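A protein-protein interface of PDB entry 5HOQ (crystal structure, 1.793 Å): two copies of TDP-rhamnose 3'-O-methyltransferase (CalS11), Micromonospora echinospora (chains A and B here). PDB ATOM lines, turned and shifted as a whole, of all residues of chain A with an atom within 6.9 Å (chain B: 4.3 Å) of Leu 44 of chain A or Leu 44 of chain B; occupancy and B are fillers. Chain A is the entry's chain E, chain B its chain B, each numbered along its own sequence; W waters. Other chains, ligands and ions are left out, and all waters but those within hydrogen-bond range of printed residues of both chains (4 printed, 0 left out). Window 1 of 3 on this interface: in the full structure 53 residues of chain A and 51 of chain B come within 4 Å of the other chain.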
ATOM      1  N   LEU A  30     -10.859  -2.447 -15.726  1.00  0.00           N
ATOM      2  CA  LEU A  30     -11.297  -2.784 -17.075  1.00  0.00           C
ATOM      3  C   LEU A  30     -12.611  -3.562 -17.047  1.00  0.00           C
ATOM      4  O   LEU A  30     -13.524  -3.295 -17.840  1.00  0.00           O
ATOM      5  CB  LEU A  30     -10.210  -3.610 -17.766  1.00  0.00           C
ATOM      6  CG  LEU A  30     -10.633  -4.301 -19.062  1.00  0.00           C
ATOM      7  CD1 LEU A  30     -11.143  -3.305 -20.074  1.00  0.00           C
ATOM      8  CD2 LEU A  30      -9.505  -5.125 -19.617  1.00  0.00           C
ATOM      9  N   GLU A  39     -17.770   0.951 -25.910  1.00  0.00           N
ATOM     10  CA  GLU A  39     -16.767   2.000 -26.050  1.00  0.00           C
ATOM     11  C   GLU A  39     -15.407   1.600 -25.495  1.00  0.00           C
ATOM     12  O   GLU A  39     -14.437   2.349 -25.668  1.00  0.00           O
ATOM     13  CB  GLU A  39     -17.242   3.283 -25.339  1.00  0.00           C
ATOM     14  CG  GLU A  39     -18.283   4.081 -26.101  1.00  0.00           C
ATOM     15  CD  GLU A  39     -17.695   4.895 -27.255  1.00  0.00           C
ATOM     16  OE1 GLU A  39     -16.472   5.228 -27.238  1.00  0.00           O
ATOM     17  OE2 GLU A  39     -18.467   5.199 -28.191  1.00  0.00           O
ATOM     18  N   LEU A  40     -15.292   0.433 -24.860  1.00  0.00           N
ATOM     19  CA  LEU A  40     -13.997   0.046 -24.304  1.00  0.00           C
ATOM     20  C   LEU A  40     -12.911  -0.022 -25.368  1.00  0.00           C
ATOM     21  O   LEU A  40     -11.775   0.387 -25.109  1.00  0.00           O
ATOM     22  CB  LEU A  40     -14.090  -1.285 -23.578  1.00  0.00           C
ATOM     23  CG  LEU A  40     -14.934  -1.238 -22.308  1.00  0.00           C
ATOM     24  CD1 LEU A  40     -15.092  -2.666 -21.784  1.00  0.00           C
ATOM     25  CD2 LEU A  40     -14.330  -0.316 -21.261  1.00  0.00           C
ATOM     26  N   VAL A  41     -13.212  -0.549 -26.560  1.00  0.00           N
ATOM     27  CA  VAL A  41     -12.165  -0.671 -27.578  1.00  0.00           C
ATOM     28  C   VAL A  41     -11.772   0.694 -28.135  1.00  0.00           C
ATOM     29  O   VAL A  41     -10.878   0.787 -28.987  1.00  0.00           O
ATOM     30  CB  VAL A  41     -12.560  -1.619 -28.727  1.00  0.00           C
ATOM     31  CG1 VAL A  41     -12.695  -3.038 -28.190  1.00  0.00           C
ATOM     32  CG2 VAL A  41     -13.805  -1.125 -29.445  1.00  0.00           C
ATOM     33  N   ASN A  42     -12.433   1.755 -27.673  1.00  0.00           N
ATOM     34  CA  ASN A  42     -12.007   3.118 -27.993  1.00  0.00           C
ATOM     35  C   ASN A  42     -11.196   3.748 -26.871  1.00  0.00           C
ATOM     36  O   ASN A  42     -10.794   4.904 -26.991  1.00  0.00           O
ATOM     37  CB  ASN A  42     -13.224   4.009 -28.325  1.00  0.00           C
ATOM     38  CG  ASN A  42     -13.984   3.510 -29.557  1.00  0.00           C
ATOM     39  OD1 ASN A  42     -13.386   2.924 -30.469  1.00  0.00           O
ATOM     40  ND2 ASN A  42     -15.303   3.714 -29.576  1.00  0.00           N
ATOM     41  N   ASN A  43     -10.947   3.012 -25.787  1.00  0.00           N
ATOM     42  CA  ASN A  43     -10.266   3.577 -24.630  1.00  0.00           C
ATOM     43  C   ASN A  43      -9.237   2.627 -24.033  1.00  0.00           C
ATOM     44  O   ASN A  43      -8.883   2.773 -22.860  1.00  0.00           O
ATOM     45  CB  ASN A  43     -11.302   3.971 -23.579  1.00  0.00           C
ATOM     46  CG  ASN A  43     -12.123   5.159 -24.011  1.00  0.00           C
ATOM     47  OD1 ASN A  43     -11.656   6.292 -23.950  1.00  0.00           O
ATOM     48  ND2 ASN A  43     -13.341   4.910 -24.474  1.00  0.00           N
ATOM     49  N   LEU A  44      -8.716   1.694 -24.828  1.00  0.00           N
ATOM     50  CA  LEU A  44      -7.790   0.702 -24.303  1.00  0.00           C
ATOM     51  C   LEU A  44      -6.541   1.322 -23.690  1.00  0.00           C
ATOM     52  O   LEU A  44      -6.003   0.730 -22.738  1.00  0.00           O
ATOM     53  CB  LEU A  44      -7.442  -0.299 -25.425  1.00  0.00           C
ATOM     54  CG  LEU A  44      -8.652  -1.071 -25.998  1.00  0.00           C
ATOM     55  CD1 LEU A  44      -8.262  -1.864 -27.255  1.00  0.00           C
ATOM     56  CD2 LEU A  44      -9.219  -2.006 -24.949  1.00  0.00           C
ATOM     57  N   PRO A  45      -6.040   2.467 -24.155  1.00  0.00           N
ATOM     58  CA  PRO A  45      -4.875   3.075 -23.487  1.00  0.00           C
ATOM     59  C   PRO A  45      -5.083   3.361 -22.004  1.00  0.00           C
ATOM     60  O   PRO A  45      -4.091   3.501 -21.283  1.00  0.00           O
ATOM     61  CB  PRO A  45      -4.656   4.364 -24.289  1.00  0.00           C
ATOM     62  CG  PRO A  45      -5.115   3.991 -25.678  1.00  0.00           C
ATOM     63  CD  PRO A  45      -6.279   3.049 -25.487  1.00  0.00           C
ATOM     64  N   LEU A  46      -6.327   3.448 -21.515  1.00  0.00           N
ATOM     65  CA  LEU A  46      -6.531   3.594 -20.080  1.00  0.00           C
ATOM     66  C   LEU A  46      -5.951   2.418 -19.303  1.00  0.00           C
ATOM     67  O   LEU A  46      -5.575   2.570 -18.131  1.00  0.00           O
ATOM     68  CB  LEU A  46      -8.032   3.739 -19.767  1.00  0.00           C
ATOM     69  CG  LEU A  46      -8.726   5.059 -20.075  1.00  0.00           C
ATOM     70  CD1 LEU A  46     -10.246   4.904 -19.845  1.00  0.00           C
ATOM     71  CD2 LEU A  46      -8.158   6.152 -19.189  1.00  0.00           C
ATOM     72  N   PHE A  47      -5.872   1.242 -19.924  1.00  0.00           N
ATOM     73  CA  PHE A  47      -5.500   0.001 -19.245  1.00  0.00           C
ATOM     74  C   PHE A  47      -4.173  -0.565 -19.732  1.00  0.00           C
ATOM     75  O   PHE A  47      -3.781  -1.661 -19.311  1.00  0.00           O
ATOM     76  CB  PHE A  47      -6.640  -1.019 -19.406  1.00  0.00           C
ATOM     77  CG  PHE A  47      -8.005  -0.412 -19.155  1.00  0.00           C
ATOM     78  CD1 PHE A  47      -8.420  -0.112 -17.869  1.00  0.00           C
ATOM     79  CD2 PHE A  47      -8.849  -0.110 -20.208  1.00  0.00           C
ATOM     80  CE1 PHE A  47      -9.666   0.477 -17.634  1.00  0.00           C
ATOM     81  CE2 PHE A  47     -10.097   0.453 -19.980  1.00  0.00           C
ATOM     82  CZ  PHE A  47     -10.494   0.765 -18.701  1.00  0.00           C
ATOM     83  N   LEU A  48      -3.451   0.190 -20.565  1.00  0.00           N
ATOM     84  CA  LEU A  48      -2.224  -0.235 -21.217  1.00  0.00           C
ATOM     85  C   LEU A  48      -1.054   0.379 -20.454  1.00  0.00           C
ATOM     86  O   LEU A  48      -0.673   1.524 -20.704  1.00  0.00           O
ATOM     87  CB  LEU A  48      -2.222   0.220 -22.675  1.00  0.00           C
ATOM     88  CG  LEU A  48      -1.033  -0.210 -23.534  1.00  0.00           C
ATOM     89  CD1 LEU A  48      -1.150  -1.665 -23.801  1.00  0.00           C
ATOM     90  CD2 LEU A  48      -0.998   0.566 -24.820  1.00  0.00           C
ATOM     91  N   ARG A  49      -0.481  -0.379 -19.520  1.00  0.00           N
ATOM     92  CA  ARG A  49       0.571   0.162 -18.664  1.00  0.00           C
ATOM     93  C   ARG A  49       1.907   0.284 -19.403  1.00  0.00           C
ATOM     94  O   ARG A  49       2.148  -0.326 -20.457  1.00  0.00           O
ATOM     95  CB  ARG A  49       0.755  -0.702 -17.423  1.00  0.00           C
ATOM     96  CG  ARG A  49       1.340  -2.086 -17.710  1.00  0.00           C
ATOM     97  CD  ARG A  49       1.229  -2.970 -16.469  1.00  0.00           C
ATOM     98  NE  ARG A  49       1.879  -4.257 -16.676  1.00  0.00           N
ATOM     99  CZ  ARG A  49       1.348  -5.274 -17.351  1.00  0.00           C
ATOM    100  NH1 ARG A  49       0.138  -5.170 -17.894  1.00  0.00           N
ATOM    101  NH2 ARG A  49       2.031  -6.407 -17.477  1.00  0.00           N
ATOM    102  N   GLN A  52       3.616  -2.696 -21.202  1.00  0.00           N
ATOM    103  CA  GLN A  52       2.975  -3.136 -22.436  1.00  0.00           C
ATOM    104  C   GLN A  52       3.020  -2.057 -23.526  1.00  0.00           C
ATOM    105  O   GLN A  52       3.190  -2.375 -24.712  1.00  0.00           O
ATOM    106  CB  GLN A  52       1.551  -3.568 -22.119  1.00  0.00           C
ATOM    107  CG  GLN A  52       1.503  -4.753 -21.138  1.00  0.00           C
ATOM    108  CD  GLN A  52       2.117  -6.030 -21.743  1.00  0.00           C
ATOM    109  OE1 GLN A  52       2.233  -6.162 -22.970  1.00  0.00           O
ATOM    110  NE2 GLN A  52       2.516  -6.965 -20.882  1.00  0.00           N
ATOM    111  N   ARG A  82      -0.443 -11.126 -29.233  1.00  0.00           N
ATOM    112  CA  ARG A  82      -0.244  -9.690 -29.027  1.00  0.00           C
ATOM    113  C   ARG A  82       0.475  -9.028 -30.212  1.00  0.00           C
ATOM    114  O   ARG A  82       0.034  -7.990 -30.716  1.00  0.00           O
ATOM    115  CB  ARG A  82       0.542  -9.476 -27.723  1.00  0.00           C
ATOM    116  CG  ARG A  82       1.123  -8.056 -27.523  1.00  0.00           C
ATOM    117  CD  ARG A  82       2.014  -7.928 -26.270  1.00  0.00           C
ATOM    118  NE  ARG A  82       3.239  -8.734 -26.348  1.00  0.00           N
ATOM    119  CZ  ARG A  82       4.225  -8.717 -25.449  1.00  0.00           C
ATOM    120  NH1 ARG A  82       4.161  -7.941 -24.385  1.00  0.00           N
ATOM    121  NH2 ARG A  82       5.291  -9.488 -25.605  1.00  0.00           N
ATOM    122  N   THR A  86      -0.880  -6.303 -33.169  1.00  0.00           N
ATOM    123  CA  THR A  86      -0.167  -5.042 -33.359  1.00  0.00           C
ATOM    124  C   THR A  86       0.191  -4.859 -34.824  1.00  0.00           C
ATOM    125  O   THR A  86      -0.034  -3.789 -35.406  1.00  0.00           O
ATOM    126  CB  THR A  86       1.092  -5.006 -32.497  1.00  0.00           C
ATOM    127  OG1 THR A  86       0.760  -5.237 -31.131  1.00  0.00           O
ATOM    128  CG2 THR A  86       1.810  -3.652 -32.609  1.00  0.00           C
ATOM    129  N   LEU B  40      -5.696 -10.332 -19.888  1.00  0.00           N
ATOM    130  CA  LEU B  40      -6.257  -9.434 -20.896  1.00  0.00           C
ATOM    131  C   LEU B  40      -5.433  -8.161 -21.043  1.00  0.00           C
ATOM    132  O   LEU B  40      -5.165  -7.713 -22.164  1.00  0.00           O
ATOM    133  CB  LEU B  40      -7.707  -9.061 -20.566  1.00  0.00           C
ATOM    134  CG  LEU B  40      -8.774 -10.083 -20.876  1.00  0.00           C
ATOM    135  CD1 LEU B  40     -10.112  -9.498 -20.436  1.00  0.00           C
ATOM    136  CD2 LEU B  40      -8.786 -10.441 -22.348  1.00  0.00           C
ATOM    137  N   VAL B  41      -5.040  -7.548 -19.931  1.00  0.00           N
ATOM    138  CA  VAL B  41      -4.320  -6.281 -20.018  1.00  0.00           C
ATOM    139  C   VAL B  41      -2.872  -6.486 -20.464  1.00  0.00           C
ATOM    140  O   VAL B  41      -2.096  -5.524 -20.543  1.00  0.00           O
ATOM    141  CB  VAL B  41      -4.382  -5.501 -18.684  1.00  0.00           C
ATOM    142  CG1 VAL B  41      -5.828  -5.186 -18.325  1.00  0.00           C
ATOM    143  CG2 VAL B  41      -3.703  -6.266 -17.551  1.00  0.00           C
ATOM    144  N   ASN B  42      -2.491  -7.734 -20.767  1.00  0.00           N
ATOM    145  CA  ASN B  42      -1.225  -7.996 -21.430  1.00  0.00           C
ATOM    146  C   ASN B  42      -1.402  -8.228 -22.916  1.00  0.00           C
ATOM    147  O   ASN B  42      -0.417  -8.504 -23.603  1.00  0.00           O
ATOM    148  CB  ASN B  42      -0.507  -9.203 -20.800  1.00  0.00           C
ATOM    149  CG  ASN B  42      -0.141  -8.952 -19.362  1.00  0.00           C
ATOM    150  OD1 ASN B  42       0.029  -7.805 -18.959  1.00  0.00           O
ATOM    151  ND2 ASN B  42      -0.051 -10.015 -18.569  1.00  0.00           N
ATOM    152  N   ASN B  43      -2.626  -8.086 -23.433  1.00  0.00           N
ATOM    153  CA  ASN B  43      -2.897  -8.405 -24.830  1.00  0.00           C
ATOM    154  C   ASN B  43      -3.858  -7.416 -25.472  1.00  0.00           C
ATOM    155  O   ASN B  43      -4.510  -7.748 -26.469  1.00  0.00           O
ATOM    156  CB  ASN B  43      -3.445  -9.828 -24.935  1.00  0.00           C
ATOM    157  CG  ASN B  43      -2.383 -10.854 -24.644  1.00  0.00           C
ATOM    158  OD1 ASN B  43      -1.542 -11.127 -25.488  1.00  0.00           O
ATOM    159  ND2 ASN B  43      -2.366 -11.369 -23.422  1.00  0.00           N
ATOM    160  N   LEU B  44      -3.952  -6.201 -24.939  1.00  0.00           N
ATOM    161  CA  LEU B  44      -4.908  -5.249 -25.478  1.00  0.00           C
ATOM    162  C   LEU B  44      -4.669  -4.908 -26.947  1.00  0.00           C
ATOM    163  O   LEU B  44      -5.654  -4.562 -27.624  1.00  0.00           O
ATOM    164  CB  LEU B  44      -4.901  -3.977 -24.613  1.00  0.00           C
ATOM    165  CG  LEU B  44      -5.183  -4.218 -23.136  1.00  0.00           C
ATOM    166  CD1 LEU B  44      -5.020  -2.923 -22.376  1.00  0.00           C
ATOM    167  CD2 LEU B  44      -6.590  -4.806 -22.907  1.00  0.00           C
ATOM    168  N   PRO B  45      -3.445  -4.959 -27.490  1.00  0.00           N
ATOM    169  CA  PRO B  45      -3.277  -4.682 -28.933  1.00  0.00           C
ATOM    170  C   PRO B  45      -4.028  -5.651 -29.837  1.00  0.00           C
ATOM    171  O   PRO B  45      -4.247  -5.334 -31.017  1.00  0.00           O
ATOM    172  CB  PRO B  45      -1.755  -4.782 -29.135  1.00  0.00           C
ATOM    173  CG  PRO B  45      -1.169  -4.382 -27.788  1.00  0.00           C
ATOM    174  CD  PRO B  45      -2.143  -5.024 -26.794  1.00  0.00           C
ATOM    175  N   LEU B  46      -4.439  -6.822 -29.329  1.00  0.00           N
ATOM    176  CA  LEU B  46      -5.340  -7.668 -30.111  1.00  0.00           C
ATOM    177  C   LEU B  46      -6.595  -6.916 -30.509  1.00  0.00           C
ATOM    178  O   LEU B  46      -7.205  -7.224 -31.543  1.00  0.00           O
ATOM    179  CB  LEU B  46      -5.730  -8.921 -29.314  1.00  0.00           C
ATOM    180  CG  LEU B  46      -4.682 -10.027 -29.117  1.00  0.00           C
ATOM    181  CD1 LEU B  46      -5.269 -11.127 -28.187  1.00  0.00           C
ATOM    182  CD2 LEU B  46      -4.287 -10.608 -30.469  1.00  0.00           C
ATOM    183  N   PHE B  47      -7.002  -5.937 -29.699  1.00  0.00           N
ATOM    184  CA  PHE B  47      -8.297  -5.287 -29.843  1.00  0.00           C
ATOM    185  C   PHE B  47      -8.180  -3.817 -30.212  1.00  0.00           C
ATOM    186  O   PHE B  47      -9.210  -3.127 -30.308  1.00  0.00           O
ATOM    187  CB  PHE B  47      -9.095  -5.461 -28.552  1.00  0.00           C
ATOM    188  CG  PHE B  47      -9.043  -6.878 -28.010  1.00  0.00           C
ATOM    189  CD1 PHE B  47      -9.735  -7.894 -28.639  1.00  0.00           C
ATOM    190  CD2 PHE B  47      -8.282  -7.181 -26.889  1.00  0.00           C
ATOM    191  CE1 PHE B  47      -9.666  -9.197 -28.171  1.00  0.00           C
ATOM    192  CE2 PHE B  47      -8.220  -8.479 -26.406  1.00  0.00           C
ATOM    193  CZ  PHE B  47      -8.912  -9.489 -27.047  1.00  0.00           C
ATOM    194  N   LEU B  48      -6.962  -3.343 -30.469  1.00  0.00           N
ATOM    195  CA  LEU B  48      -6.661  -1.957 -30.818  1.00  0.00           C
ATOM    196  C   LEU B  48      -6.568  -1.826 -32.338  1.00  0.00           C
ATOM    197  O   LEU B  48      -5.534  -2.130 -32.939  1.00  0.00           O
ATOM    198  CB  LEU B  48      -5.348  -1.547 -30.157  1.00  0.00           C
ATOM    199  CG  LEU B  48      -4.897  -0.090 -30.283  1.00  0.00           C
ATOM    200  CD1 LEU B  48      -5.812   0.819 -29.500  1.00  0.00           C
ATOM    201  CD2 LEU B  48      -3.469   0.050 -29.797  1.00  0.00           C
HETATM  202  O   HOH W   1       0.280  -5.690 -24.826  1.00  0.00           O
HETATM  203  O   HOH W   2     -10.006  -0.741 -31.123  1.00  0.00           O
HETATM  204  O   HOH W   3       0.465 -12.497 -26.565  1.00  0.00           O
HETATM  205  O   HOH W   4      -1.634  -3.092 -19.265  1.00  0.00           O
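Of chain B, only Leu 44, Phe 47 and Leu 48 come within 4 Å of Leu 44 of chain A.
Of chain A, only Leu 44 (3.8 Å), Phe 47 (3.5 Å) and Leu 48 (3.9 Å) come within 4 Å of Leu 44 of chain B.
Of the printed residues of chain B, Arg 49 of chain A touches Val 41 and Asn 42.
Of the printed residues of chain A, Asn 43 of chain B touches Arg 82 (3.5 Å).
Of the printed residues of chain B, Arg 82 of chain A touches Asn 42 (3.7 Å), Asn 43 (3.5 Å) and Pro 45 (3.999 Å).
Of the printed residues of chain B, Phe 47 of chain A touches Val 41 and Leu 44.
Glu 39 of chain A touches none of the printed residues of chain B.
NE2 of Gln 52 of chain A sits at hydrogen-bond distance from OD1 of Asn 42 of chain B, 3.3 Å away.
OD1 of Asn 42 of chain B lies within hydrogen-bond range of NH1 of Arg 49 of chain A, 2.8 Å away.
The backbone carbonyl oxygen (O) of Val 41 of chain B is in hydrogen-bond range of the guanidinium group (NH1) of Arg 49 of chain A.
Water W4 lies within hydrogen-bond range of O of Phe 47 of chain A (2.6 Å), O of Val 41 of chain B (2.8 Å) and N of Arg 49 of chain A (3.0 Å).
Water W2 bridges O of Phe 47 of chain B and O of Val 41 of chain A.
Water W3 lies within hydrogen-bond range of OD1 of Asn 43 of chain B and N of Arg 82 of chain A.
Water W1 bridges the side-chain amide oxygen of Gln 52 of chain A (2.7 Å) and the backbone carbonyl oxygen of Asn 42 of chain B (3.1 Å).
Among the printed residues, pairs that only touch across the chains: Leu 30 of chain A with Val 41 of chain B, Val 41 of chain A with Phe 47 of chain B, Leu 44 of chain A with Leu 44 of chain B, Leu 44 of chain A with Phe 47 of chain B, Leu 44 of chain A with Leu 48 of chain B, Phe 47 of chain A with Val 41 of chain B, Phe 47 of chain A with Leu 44 of chain B, Leu 48 of chain A with Leu 44 of chain B, Gln 52 of chain A with Val 41 of chain B, Arg 82 of chain A with Asn 42 of chain B, Arg 82 of chain A with Asn 43 of chain B, Arg 82 of chain A with Pro 45 of chain B and Thr 86 of chain A with Pro 45 of chain B.
Of the 9 printed residues of chain B, 7 touch a printed residue of chain A.
Printed residues of chain B that touch a printed residue of chain A: Val 41, Asn 42, Asn 43, Leu 44, Pro 45, Phe 47 and Leu 48.
Hydrophobic or aromatic side chains of chain B within 4 Å of the printed part of chain A: Val 41, Leu 44, Pro 45 and Phe 47.
Of the 15 printed residues of chain A, 9 touch a printed residue of chain B.
NH1 of Arg 82 of chain A is in hydrogen-bond range of OE1 of Gln 52 of chain A.
The backbone carbonyl oxygen of Arg 82 of chain A lies within hydrogen-bond range of the side-chain hydroxyl of Thr 86 of chain A (2.9 Å).
NH2 of Arg 49 of chain A lies close to NE2 of Gln 52 of chain A (3.5 Å).
Val 41 of chain A touches Phe 47 of chain B, and with the chains exchanged Phe 47 of chain A touches Val 41 of chain B.
Leu 44 of chain A touches its own counterpart, Leu 44 of chain B.
Leu 44 of chain A touches Phe 47 of chain B, and with the chains exchanged Phe 47 of chain A touches Leu 44 of chain B.
Leu 44 of chain A touches Leu 48 of chain B, and with the chains exchanged Leu 48 of chain A touches Leu 44 of chain B.
Positions printed for both chains: 40, 41, 42, 43, 44, 45, 46, 47 and 48.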
